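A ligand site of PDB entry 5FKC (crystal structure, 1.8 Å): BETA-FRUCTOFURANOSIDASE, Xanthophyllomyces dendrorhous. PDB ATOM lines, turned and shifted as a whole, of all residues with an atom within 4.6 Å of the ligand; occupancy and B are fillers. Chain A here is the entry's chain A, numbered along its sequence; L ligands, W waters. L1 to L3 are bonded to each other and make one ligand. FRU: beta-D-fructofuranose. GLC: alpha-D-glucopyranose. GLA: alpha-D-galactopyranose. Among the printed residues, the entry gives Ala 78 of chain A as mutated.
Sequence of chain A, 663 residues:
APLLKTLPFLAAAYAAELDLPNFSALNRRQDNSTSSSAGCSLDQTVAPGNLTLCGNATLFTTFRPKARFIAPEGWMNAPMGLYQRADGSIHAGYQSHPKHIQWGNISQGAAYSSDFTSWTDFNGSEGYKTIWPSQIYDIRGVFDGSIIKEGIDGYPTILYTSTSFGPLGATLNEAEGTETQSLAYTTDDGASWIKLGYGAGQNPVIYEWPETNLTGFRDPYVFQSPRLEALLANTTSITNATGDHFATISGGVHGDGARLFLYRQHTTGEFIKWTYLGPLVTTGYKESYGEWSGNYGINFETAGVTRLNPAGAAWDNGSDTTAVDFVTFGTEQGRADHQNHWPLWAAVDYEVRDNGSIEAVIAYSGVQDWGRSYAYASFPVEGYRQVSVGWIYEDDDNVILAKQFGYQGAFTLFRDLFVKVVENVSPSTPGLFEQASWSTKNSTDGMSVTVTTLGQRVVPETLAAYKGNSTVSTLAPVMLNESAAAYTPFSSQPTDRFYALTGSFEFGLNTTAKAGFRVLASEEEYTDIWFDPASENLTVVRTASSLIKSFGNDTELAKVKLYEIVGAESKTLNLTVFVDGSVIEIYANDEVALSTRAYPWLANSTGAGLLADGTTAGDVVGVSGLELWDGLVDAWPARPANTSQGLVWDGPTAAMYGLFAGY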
ATOM      1  N   ASN A  77      26.872  23.983 -36.943  1.00  0.00           N
ATOM      2  CA  ASN A  77      26.228  24.010 -35.645  1.00  0.00           C
ATOM      3  C   ASN A  77      26.631  25.252 -34.836  1.00  0.00           C
ATOM      4  O   ASN A  77      26.339  26.366 -35.267  1.00  0.00           O
ATOM      5  CB  ASN A  77      26.252  22.643 -34.895  1.00  0.00           C
ATOM      6  CG  ASN A  77      27.646  22.070 -34.655  1.00  0.00           C
ATOM      7  OD1 ASN A  77      28.369  21.726 -35.578  1.00  0.00           O
ATOM      8  ND2 ASN A  77      27.982  21.899 -33.379  1.00  0.00           N
ATOM      9  N   ALA A  78      27.288  25.084 -33.688  1.00  0.00           N
ATOM     10  CA  ALA A  78      27.452  26.154 -32.699  1.00  0.00           C
ATOM     11  C   ALA A  78      28.198  27.367 -33.237  1.00  0.00           C
ATOM     12  O   ALA A  78      29.220  27.216 -33.901  1.00  0.00           O
ATOM     13  CB  ALA A  78      28.203  25.621 -31.488  1.00  0.00           C
ATOM     14  N   GLN A  95      30.889  26.253 -36.011  1.00  0.00           N
ATOM     15  CA  GLN A  95      31.224  24.861 -36.225  1.00  0.00           C
ATOM     16  C   GLN A  95      30.723  24.486 -37.625  1.00  0.00           C
ATOM     17  O   GLN A  95      29.543  24.703 -37.912  1.00  0.00           O
ATOM     18  CB  GLN A  95      30.564  23.984 -35.153  1.00  0.00           C
ATOM     19  CG  GLN A  95      31.129  24.214 -33.750  1.00  0.00           C
ATOM     20  CD  GLN A  95      32.446  23.505 -33.538  1.00  0.00           C
ATOM     21  OE1 GLN A  95      32.473  22.339 -33.200  1.00  0.00           O
ATOM     22  NE2 GLN A  95      33.557  24.227 -33.749  1.00  0.00           N
ATOM     23  N   TRP A 103      27.629  16.134 -38.980  1.00  0.00           N
ATOM     24  CA  TRP A 103      28.820  16.632 -38.298  1.00  0.00           C
ATOM     25  C   TRP A 103      30.058  15.791 -38.594  1.00  0.00           C
ATOM     26  O   TRP A 103      29.980  14.577 -38.756  1.00  0.00           O
ATOM     27  CB  TRP A 103      28.510  16.619 -36.797  1.00  0.00           C
ATOM     28  CG  TRP A 103      29.521  17.158 -35.834  1.00  0.00           C
ATOM     29  CD1 TRP A 103      29.501  18.386 -35.243  1.00  0.00           C
ATOM     30  CD2 TRP A 103      30.641  16.467 -35.277  1.00  0.00           C
ATOM     31  NE1 TRP A 103      30.546  18.512 -34.363  1.00  0.00           N
ATOM     32  CE2 TRP A 103      31.268  17.349 -34.360  1.00  0.00           C
ATOM     33  CE3 TRP A 103      31.171  15.185 -35.448  1.00  0.00           C
ATOM     34  CZ2 TRP A 103      32.397  16.995 -33.639  1.00  0.00           C
ATOM     35  CZ3 TRP A 103      32.300  14.831 -34.727  1.00  0.00           C
ATOM     36  CH2 TRP A 103      32.897  15.731 -33.821  1.00  0.00           C
ATOM     37  N   ILE A 106      35.259  18.757 -37.624  1.00  0.00           N
ATOM     38  CA  ILE A 106      34.568  19.999 -37.352  1.00  0.00           C
ATOM     39  C   ILE A 106      35.588  21.141 -37.279  1.00  0.00           C
ATOM     40  O   ILE A 106      36.661  21.004 -36.705  1.00  0.00           O
ATOM     41  CB  ILE A 106      33.619  19.887 -36.144  1.00  0.00           C
ATOM     42  CG1 ILE A 106      32.479  20.914 -36.261  1.00  0.00           C
ATOM     43  CG2 ILE A 106      34.369  20.003 -34.820  1.00  0.00           C
ATOM     44  CD1 ILE A 106      31.445  20.596 -37.331  1.00  0.00           C
ATOM     45  N   ARG A 140      40.593  15.316 -34.280  1.00  0.00           N
ATOM     46  CA  ARG A 140      39.243  14.790 -34.172  1.00  0.00           C
ATOM     47  C   ARG A 140      38.181  15.887 -34.259  1.00  0.00           C
ATOM     48  O   ARG A 140      36.999  15.584 -34.340  1.00  0.00           O
ATOM     49  CB  ARG A 140      39.111  13.978 -32.880  1.00  0.00           C
ATOM     50  CG  ARG A 140      37.845  13.141 -32.766  1.00  0.00           C
ATOM     51  CD  ARG A 140      36.827  13.706 -31.807  1.00  0.00           C
ATOM     52  NE  ARG A 140      35.797  12.716 -31.552  1.00  0.00           N
ATOM     53  CZ  ARG A 140      35.917  11.675 -30.726  1.00  0.00           C
ATOM     54  NH1 ARG A 140      37.054  11.460 -30.046  1.00  0.00           N
ATOM     55  NH2 ARG A 140      34.905  10.827 -30.588  1.00  0.00           N
ATOM     56  N   PHE A 143      36.625  22.111 -31.848  1.00  0.00           N
ATOM     57  CA  PHE A 143      35.340  22.351 -31.182  1.00  0.00           C
ATOM     58  C   PHE A 143      35.208  23.849 -30.838  1.00  0.00           C
ATOM     59  O   PHE A 143      36.037  24.672 -31.266  1.00  0.00           O
ATOM     60  CB  PHE A 143      35.214  21.473 -29.919  1.00  0.00           C
ATOM     61  CG  PHE A 143      34.793  20.048 -30.165  1.00  0.00           C
ATOM     62  CD1 PHE A 143      35.177  19.341 -31.295  1.00  0.00           C
ATOM     63  CD2 PHE A 143      34.052  19.382 -29.193  1.00  0.00           C
ATOM     64  CE1 PHE A 143      34.824  18.013 -31.463  1.00  0.00           C
ATOM     65  CE2 PHE A 143      33.682  18.050 -29.359  1.00  0.00           C
ATOM     66  CZ  PHE A 143      34.063  17.368 -30.511  1.00  0.00           C
ATOM     67  N   ASP A 144      34.154  24.205 -30.120  1.00  0.00           N
ATOM     68  CA  ASP A 144      33.860  25.591 -29.735  1.00  0.00           C
ATOM     69  C   ASP A 144      35.064  26.250 -29.028  1.00  0.00           C
ATOM     70  O   ASP A 144      35.862  25.596 -28.360  1.00  0.00           O
ATOM     71  CB  ASP A 144      32.612  25.587 -28.829  1.00  0.00           C
ATOM     72  CG  ASP A 144      32.063  26.974 -28.516  1.00  0.00           C
ATOM     73  OD1 ASP A 144      32.328  27.966 -29.227  1.00  0.00           O
ATOM     74  OD2 ASP A 144      31.272  27.031 -27.519  1.00  0.00           O
ATOM     75  N   LEU A 168      34.017  10.084 -26.660  1.00  0.00           N
ATOM     76  CA  LEU A 168      33.791  11.476 -26.317  1.00  0.00           C
ATOM     77  C   LEU A 168      32.290  11.656 -26.140  1.00  0.00           C
ATOM     78  O   LEU A 168      31.509  11.460 -27.085  1.00  0.00           O
ATOM     79  CB  LEU A 168      34.333  12.391 -27.421  1.00  0.00           C
ATOM     80  CG  LEU A 168      34.475  13.898 -27.104  1.00  0.00           C
ATOM     81  CD1 LEU A 168      35.325  14.572 -28.177  1.00  0.00           C
ATOM     82  CD2 LEU A 168      33.131  14.584 -26.965  1.00  0.00           C
ATOM     83  N   GLY A 169      31.866  12.003 -24.927  1.00  0.00           N
ATOM     84  CA  GLY A 169      30.451  12.229 -24.662  1.00  0.00           C
ATOM     85  C   GLY A 169      30.070  12.035 -23.226  1.00  0.00           C
ATOM     86  O   GLY A 169      30.713  11.251 -22.502  1.00  0.00           O
ATOM     87  N   LEU A 172      29.253   8.428 -22.438  1.00  0.00           N
ATOM     88  CA  LEU A 172      30.324   7.482 -22.720  1.00  0.00           C
ATOM     89  C   LEU A 172      31.377   7.569 -21.628  1.00  0.00           C
ATOM     90  O   LEU A 172      31.269   8.377 -20.714  1.00  0.00           O
ATOM     91  CB  LEU A 172      30.944   7.790 -24.082  1.00  0.00           C
ATOM     92  CG  LEU A 172      29.983   7.716 -25.263  1.00  0.00           C
ATOM     93  CD1 LEU A 172      30.698   8.091 -26.554  1.00  0.00           C
ATOM     94  CD2 LEU A 172      29.372   6.315 -25.374  1.00  0.00           C
ATOM     95  N   ARG A 218      34.976  20.961 -22.194  1.00  0.00           N
ATOM     96  CA  ARG A 218      35.022  21.709 -23.445  1.00  0.00           C
ATOM     97  C   ARG A 218      34.380  23.083 -23.390  1.00  0.00           C
ATOM     98  O   ARG A 218      33.797  23.480 -22.356  1.00  0.00           O
ATOM     99  CB  ARG A 218      34.403  20.871 -24.576  1.00  0.00           C
ATOM    100  CG  ARG A 218      32.955  20.439 -24.368  1.00  0.00           C
ATOM    101  CD  ARG A 218      32.360  19.886 -25.670  1.00  0.00           C
ATOM    102  NE  ARG A 218      31.089  19.200 -25.432  1.00  0.00           N
ATOM    103  CZ  ARG A 218      30.957  17.985 -24.884  1.00  0.00           C
ATOM    104  NH1 ARG A 218      32.024  17.268 -24.528  1.00  0.00           N
ATOM    105  NH2 ARG A 218      29.742  17.488 -24.665  1.00  0.00           N
ATOM    106  N   ASP A 219      34.511  23.795 -24.502  1.00  0.00           N
ATOM    107  CA  ASP A 219      33.817  25.047 -24.754  1.00  0.00           C
ATOM    108  C   ASP A 219      34.350  26.156 -23.838  1.00  0.00           C
ATOM    109  O   ASP A 219      33.586  26.776 -23.099  1.00  0.00           O
ATOM    110  CB  ASP A 219      32.297  24.875 -24.646  1.00  0.00           C
ATOM    111  CG  ASP A 219      31.749  23.758 -25.547  1.00  0.00           C
ATOM    112  OD1 ASP A 219      32.473  23.329 -26.474  1.00  0.00           O
ATOM    113  OD2 ASP A 219      30.611  23.313 -25.304  1.00  0.00           O
ATOM    114  N   GLU A 301      27.285  22.492 -21.568  1.00  0.00           N
ATOM    115  CA  GLU A 301      28.004  22.836 -22.795  1.00  0.00           C
ATOM    116  C   GLU A 301      27.871  24.329 -23.063  1.00  0.00           C
ATOM    117  O   GLU A 301      26.930  24.970 -22.585  1.00  0.00           O
ATOM    118  CB  GLU A 301      27.438  22.065 -23.983  1.00  0.00           C
ATOM    119  CG  GLU A 301      27.500  20.548 -23.837  1.00  0.00           C
ATOM    120  CD  GLU A 301      26.884  19.846 -25.017  1.00  0.00           C
ATOM    121  OE1 GLU A 301      25.696  20.090 -25.309  1.00  0.00           O
ATOM    122  OE2 GLU A 301      27.575  19.027 -25.638  1.00  0.00           O
ATOM    123  N   THR A 302      28.787  24.850 -23.865  1.00  0.00           N
ATOM    124  CA  THR A 302      28.795  26.233 -24.352  1.00  0.00           C
ATOM    125  C   THR A 302      28.412  27.266 -23.301  1.00  0.00           C
ATOM    126  O   THR A 302      27.683  28.203 -23.599  1.00  0.00           O
ATOM    127  CB  THR A 302      27.923  26.425 -25.640  1.00  0.00           C
ATOM    128  OG1 THR A 302      26.527  26.411 -25.310  1.00  0.00           O
ATOM    129  CG2 THR A 302      28.214  25.344 -26.666  1.00  0.00           C
ATOM    130  N   GLU A 332      22.633  18.825 -21.191  1.00  0.00           N
ATOM    131  CA  GLU A 332      22.393  17.604 -21.934  1.00  0.00           C
ATOM    132  C   GLU A 332      21.696  16.542 -21.087  1.00  0.00           C
ATOM    133  O   GLU A 332      21.962  16.414 -19.897  1.00  0.00           O
ATOM    134  CB  GLU A 332      23.700  16.980 -22.393  1.00  0.00           C
ATOM    135  CG  GLU A 332      24.660  17.904 -23.100  1.00  0.00           C
ATOM    136  CD  GLU A 332      25.676  17.100 -23.884  1.00  0.00           C
ATOM    137  OE1 GLU A 332      25.365  16.772 -25.050  1.00  0.00           O
ATOM    138  OE2 GLU A 332      26.762  16.799 -23.327  1.00  0.00           O
ATOM    139  N   HIS A 341      18.485  18.678 -25.334  1.00  0.00           N
ATOM    140  CA  HIS A 341      19.256  19.890 -25.101  1.00  0.00           C
ATOM    141  C   HIS A 341      18.405  21.067 -24.624  1.00  0.00           C
ATOM    142  O   HIS A 341      17.451  21.455 -25.307  1.00  0.00           O
ATOM    143  CB  HIS A 341      19.964  20.309 -26.393  1.00  0.00           C
ATOM    144  CG  HIS A 341      21.280  19.651 -26.616  1.00  0.00           C
ATOM    145  ND1 HIS A 341      21.815  19.459 -27.878  1.00  0.00           N
ATOM    146  CD2 HIS A 341      22.183  19.130 -25.754  1.00  0.00           C
ATOM    147  CE1 HIS A 341      22.988  18.870 -27.781  1.00  0.00           C
ATOM    148  NE2 HIS A 341      23.241  18.656 -26.503  1.00  0.00           N
ATOM    149  N   TYR A 374      20.098  26.043 -29.609  1.00  0.00           N
ATOM    150  CA  TYR A 374      21.068  25.596 -28.630  1.00  0.00           C
ATOM    151  C   TYR A 374      22.384  26.297 -28.910  1.00  0.00           C
ATOM    152  O   TYR A 374      22.528  26.950 -29.953  1.00  0.00           O
ATOM    153  CB  TYR A 374      21.263  24.082 -28.735  1.00  0.00           C
ATOM    154  CG  TYR A 374      21.961  23.432 -27.565  1.00  0.00           C
ATOM    155  CD1 TYR A 374      21.419  23.498 -26.282  1.00  0.00           C
ATOM    156  CD2 TYR A 374      23.170  22.764 -27.741  1.00  0.00           C
ATOM    157  CE1 TYR A 374      22.050  22.900 -25.203  1.00  0.00           C
ATOM    158  CE2 TYR A 374      23.812  22.167 -26.672  1.00  0.00           C
ATOM    159  CZ  TYR A 374      23.246  22.245 -25.403  1.00  0.00           C
ATOM    160  OH  TYR A 374      23.866  21.640 -24.339  1.00  0.00           O
ATOM    161  N   TRP A 391      22.334  28.652 -32.313  1.00  0.00           N
ATOM    162  CA  TRP A 391      22.190  27.828 -33.507  1.00  0.00           C
ATOM    163  C   TRP A 391      20.809  27.208 -33.521  1.00  0.00           C
ATOM    164  O   TRP A 391      20.383  26.654 -32.507  1.00  0.00           O
ATOM    165  CB  TRP A 391      23.263  26.752 -33.491  1.00  0.00           C
ATOM    166  CG  TRP A 391      22.990  25.451 -34.201  1.00  0.00           C
ATOM    167  CD1 TRP A 391      22.846  25.259 -35.529  1.00  0.00           C
ATOM    168  CD2 TRP A 391      22.936  24.161 -33.585  1.00  0.00           C
ATOM    169  NE1 TRP A 391      22.681  23.920 -35.796  1.00  0.00           N
ATOM    170  CE2 TRP A 391      22.734  23.221 -34.616  1.00  0.00           C
ATOM    171  CE3 TRP A 391      23.032  23.700 -32.264  1.00  0.00           C
ATOM    172  CZ2 TRP A 391      22.620  21.854 -34.375  1.00  0.00           C
ATOM    173  CZ3 TRP A 391      22.918  22.333 -32.023  1.00  0.00           C
ATOM    174  CH2 TRP A 391      22.710  21.428 -33.065  1.00  0.00           C
HETATM  175  C1  FRU L   1      27.240  21.638 -28.454  1.00  0.00           C
HETATM  176  C2  FRU L   1      28.588  21.050 -28.880  1.00  0.00           C
HETATM  177  C3  FRU L   1      29.700  21.786 -28.123  1.00  0.00           C
HETATM  178  C4  FRU L   1      30.927  21.427 -28.959  1.00  0.00           C
HETATM  179  C5  FRU L   1      30.342  21.475 -30.377  1.00  0.00           C
HETATM  180  C6  FRU L   1      30.951  20.432 -31.316  1.00  0.00           C
HETATM  181  O1  FRU L   1      26.116  21.033 -29.100  1.00  0.00           O
HETATM  182  O2  FRU L   1      28.664  19.642 -28.620  1.00  0.00           O
HETATM  183  O3  FRU L   1      29.771  21.403 -26.751  1.00  0.00           O
HETATM  184  O4  FRU L   1      32.027  22.351 -28.811  1.00  0.00           O
HETATM  185  O5  FRU L   1      28.932  21.291 -30.241  1.00  0.00           O
HETATM  186  O6  FRU L   1      30.631  20.717 -32.695  1.00  0.00           O
HETATM  187  C1  GLC L   2      27.923  18.740 -29.454  1.00  0.00           C
HETATM  188  C2  GLC L   2      26.996  17.852 -28.614  1.00  0.00           C
HETATM  189  C3  GLC L   2      27.785  16.869 -27.754  1.00  0.00           C
HETATM  190  C4  GLC L   2      28.687  16.050 -28.657  1.00  0.00           C
HETATM  191  C5  GLC L   2      29.579  16.969 -29.511  1.00  0.00           C
HETATM  192  C6  GLC L   2      30.331  16.157 -30.556  1.00  0.00           C
HETATM  193  O2  GLC L   2      26.121  18.654 -27.805  1.00  0.00           O
HETATM  194  O3  GLC L   2      26.874  16.032 -27.030  1.00  0.00           O
HETATM  195  O4  GLC L   2      29.522  15.184 -27.897  1.00  0.00           O
HETATM  196  O5  GLC L   2      28.812  17.944 -30.212  1.00  0.00           O
HETATM  197  O6  GLC L   2      29.359  15.379 -31.255  1.00  0.00           O
HETATM  198  C1  GLA L   3      29.850  14.550 -32.293  1.00  0.00           C
HETATM  199  C2  GLA L   3      28.696  13.937 -33.086  1.00  0.00           C
HETATM  200  C3  GLA L   3      27.880  13.021 -32.186  1.00  0.00           C
HETATM  201  C4  GLA L   3      28.789  11.958 -31.554  1.00  0.00           C
HETATM  202  C5  GLA L   3      30.001  12.622 -30.869  1.00  0.00           C
HETATM  203  C6  GLA L   3      31.063  11.654 -30.358  1.00  0.00           C
HETATM  204  O2  GLA L   3      27.879  14.974 -33.615  1.00  0.00           O
HETATM  205  O3  GLA L   3      26.818  12.432 -32.966  1.00  0.00           O
HETATM  206  O4  GLA L   3      29.197  11.029 -32.578  1.00  0.00           O
HETATM  207  O5  GLA L   3      30.674  13.528 -31.776  1.00  0.00           O
HETATM  208  O6  GLA L   3      30.485  10.846 -29.341  1.00  0.00           O
HETATM  209  O   HOH W   1      33.174  12.271 -32.789  1.00  0.00           O
HETATM  210  O   HOH W   2      30.196  11.325 -35.108  1.00  0.00           O
HETATM  211  O   HOH W   3      30.470   8.731 -32.493  1.00  0.00           O
HETATM  212  O   HOH W   4      25.509  14.643 -34.803  1.00  0.00           O
HETATM  213  O   HOH W   5      25.925  22.244 -31.418  1.00  0.00           O
HETATM  214  O   HOH W   6      28.520  12.796 -27.415  1.00  0.00           O
HETATM  215  O   HOH W   7      28.155  14.855 -24.615  1.00  0.00           O
HETATM  216  O   HOH W   8      27.275   9.403 -33.828  1.00  0.00           O
HETATM  217  O   HOH W   9      32.845   8.872 -29.098  1.00  0.00           O
HETATM  218  O   HOH W  10      27.050  17.235 -32.380  1.00  0.00           O
HETATM  219  O   HOH W  11      25.347  14.545 -28.658  1.00  0.00           O
HETATM  220  O   HOH W  12      28.493   8.722 -29.687  1.00  0.00           O
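A ring nitrogen (NE2) of His 341 lies close to an oxygen (O2) of GLC L2. The guanidinium group of Arg 218 is in hydrogen-bond range of an oxygen (O3) of FRU L1, 2.9 Å away. The side-chain carboxylate (OD2) of Asp 219 lies within hydrogen-bond range of an oxygen (O3) of FRU L1, 2.5 Å away. An oxygen (O6) of FRU L1 is in hydrogen-bond range of the indole nitrogen of Trp 103 (2.8 Å). The backbone carbonyl oxygen of Leu 168 sits at hydrogen-bond distance from an oxygen (O6) of GLA L3 (2.6 Å). An oxygen (O6) of FRU L1 sits at hydrogen-bond distance from the side-chain amide oxygen of Gln 95, at 2.5 Å. An oxygen (O4) of FRU L1 is in hydrogen-bond range of the backbone NH of Asp 144, at 3.1 Å. An oxygen (O3) of GLC L2 is in hydrogen-bond range of the side-chain carboxylate of Glu 332 (2.6 Å). An oxygen (O2) of GLC L2 sits at hydrogen-bond distance from the side-chain carboxylate (OE2) of Glu 301 (2.6 Å). ND2 of Asn 77 sits at hydrogen-bond distance from O6 of FRU L1, at 3.0 Å.
N of Gln 95 sits at hydrogen-bond distance from O of Ala 78 (2.9 Å). O of Tyr 374 is in hydrogen-bond range of N of Trp 391 (2.9 Å). The guanidinium group (NH2) of Arg 218 is in salt-bridge range of the side-chain carboxylate (OE2) of Glu 332 (3.3 Å). The side-chain carboxylate (OE1) of Glu 301 is in hydrogen-bond range of a ring nitrogen (NE2) of His 341 (3.1 Å). O of Gln 95 is in hydrogen-bond range of N of Asn 77. The side-chain carboxylate of Glu 301 lies within hydrogen-bond range of the side-chain hydroxyl of Tyr 374, 2.6 Å away. The side-chain carboxylate (OD2) of Asp 219 is in hydrogen-bond range of the backbone NH (N) of Thr 302 (2.8 Å). The side-chain carboxylate of Glu 301 lies within salt-bridge range of the guanidinium group of Arg 218 (2.8 Å).
NH2 of Arg 140 touches C6 of GLA L3, at 3.9 Å. CB of Phe 143 touches O4 of FRU L1 (3.5 Å). CD1 of Leu 172 touches O6 of GLA L3 (3.9 Å). CE2 of Tyr 374 touches O1 of FRU L1, at 3.5 Å. Along chain A the residues within 4 Å of the ligand span positions 77 to 374.
Water W5 bridges O1 of FRU L1 and ND2 of Asn 77. Water W6 lies within hydrogen-bond range of an oxygen (O4) of GLC L2 (2.6 Å) and the backbone carbonyl oxygen (O) of Leu 168 (3.3 Å). Water W1 bridges the guanidinium group (NE) of Arg 140 and an oxygen (O5) of GLA L3. Water W7 lies within hydrogen-bond range of the side-chain carboxylate of Glu 332 (2.7 Å), an oxygen (O3) of GLC L2 (3.0 Å) and the guanidinium group of Arg 218 (3.1 Å). Water W9 lies within hydrogen-bond range of the backbone NH of Leu 168, an oxygen (O6) of GLA L3 and the guanidinium group of Arg 140.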
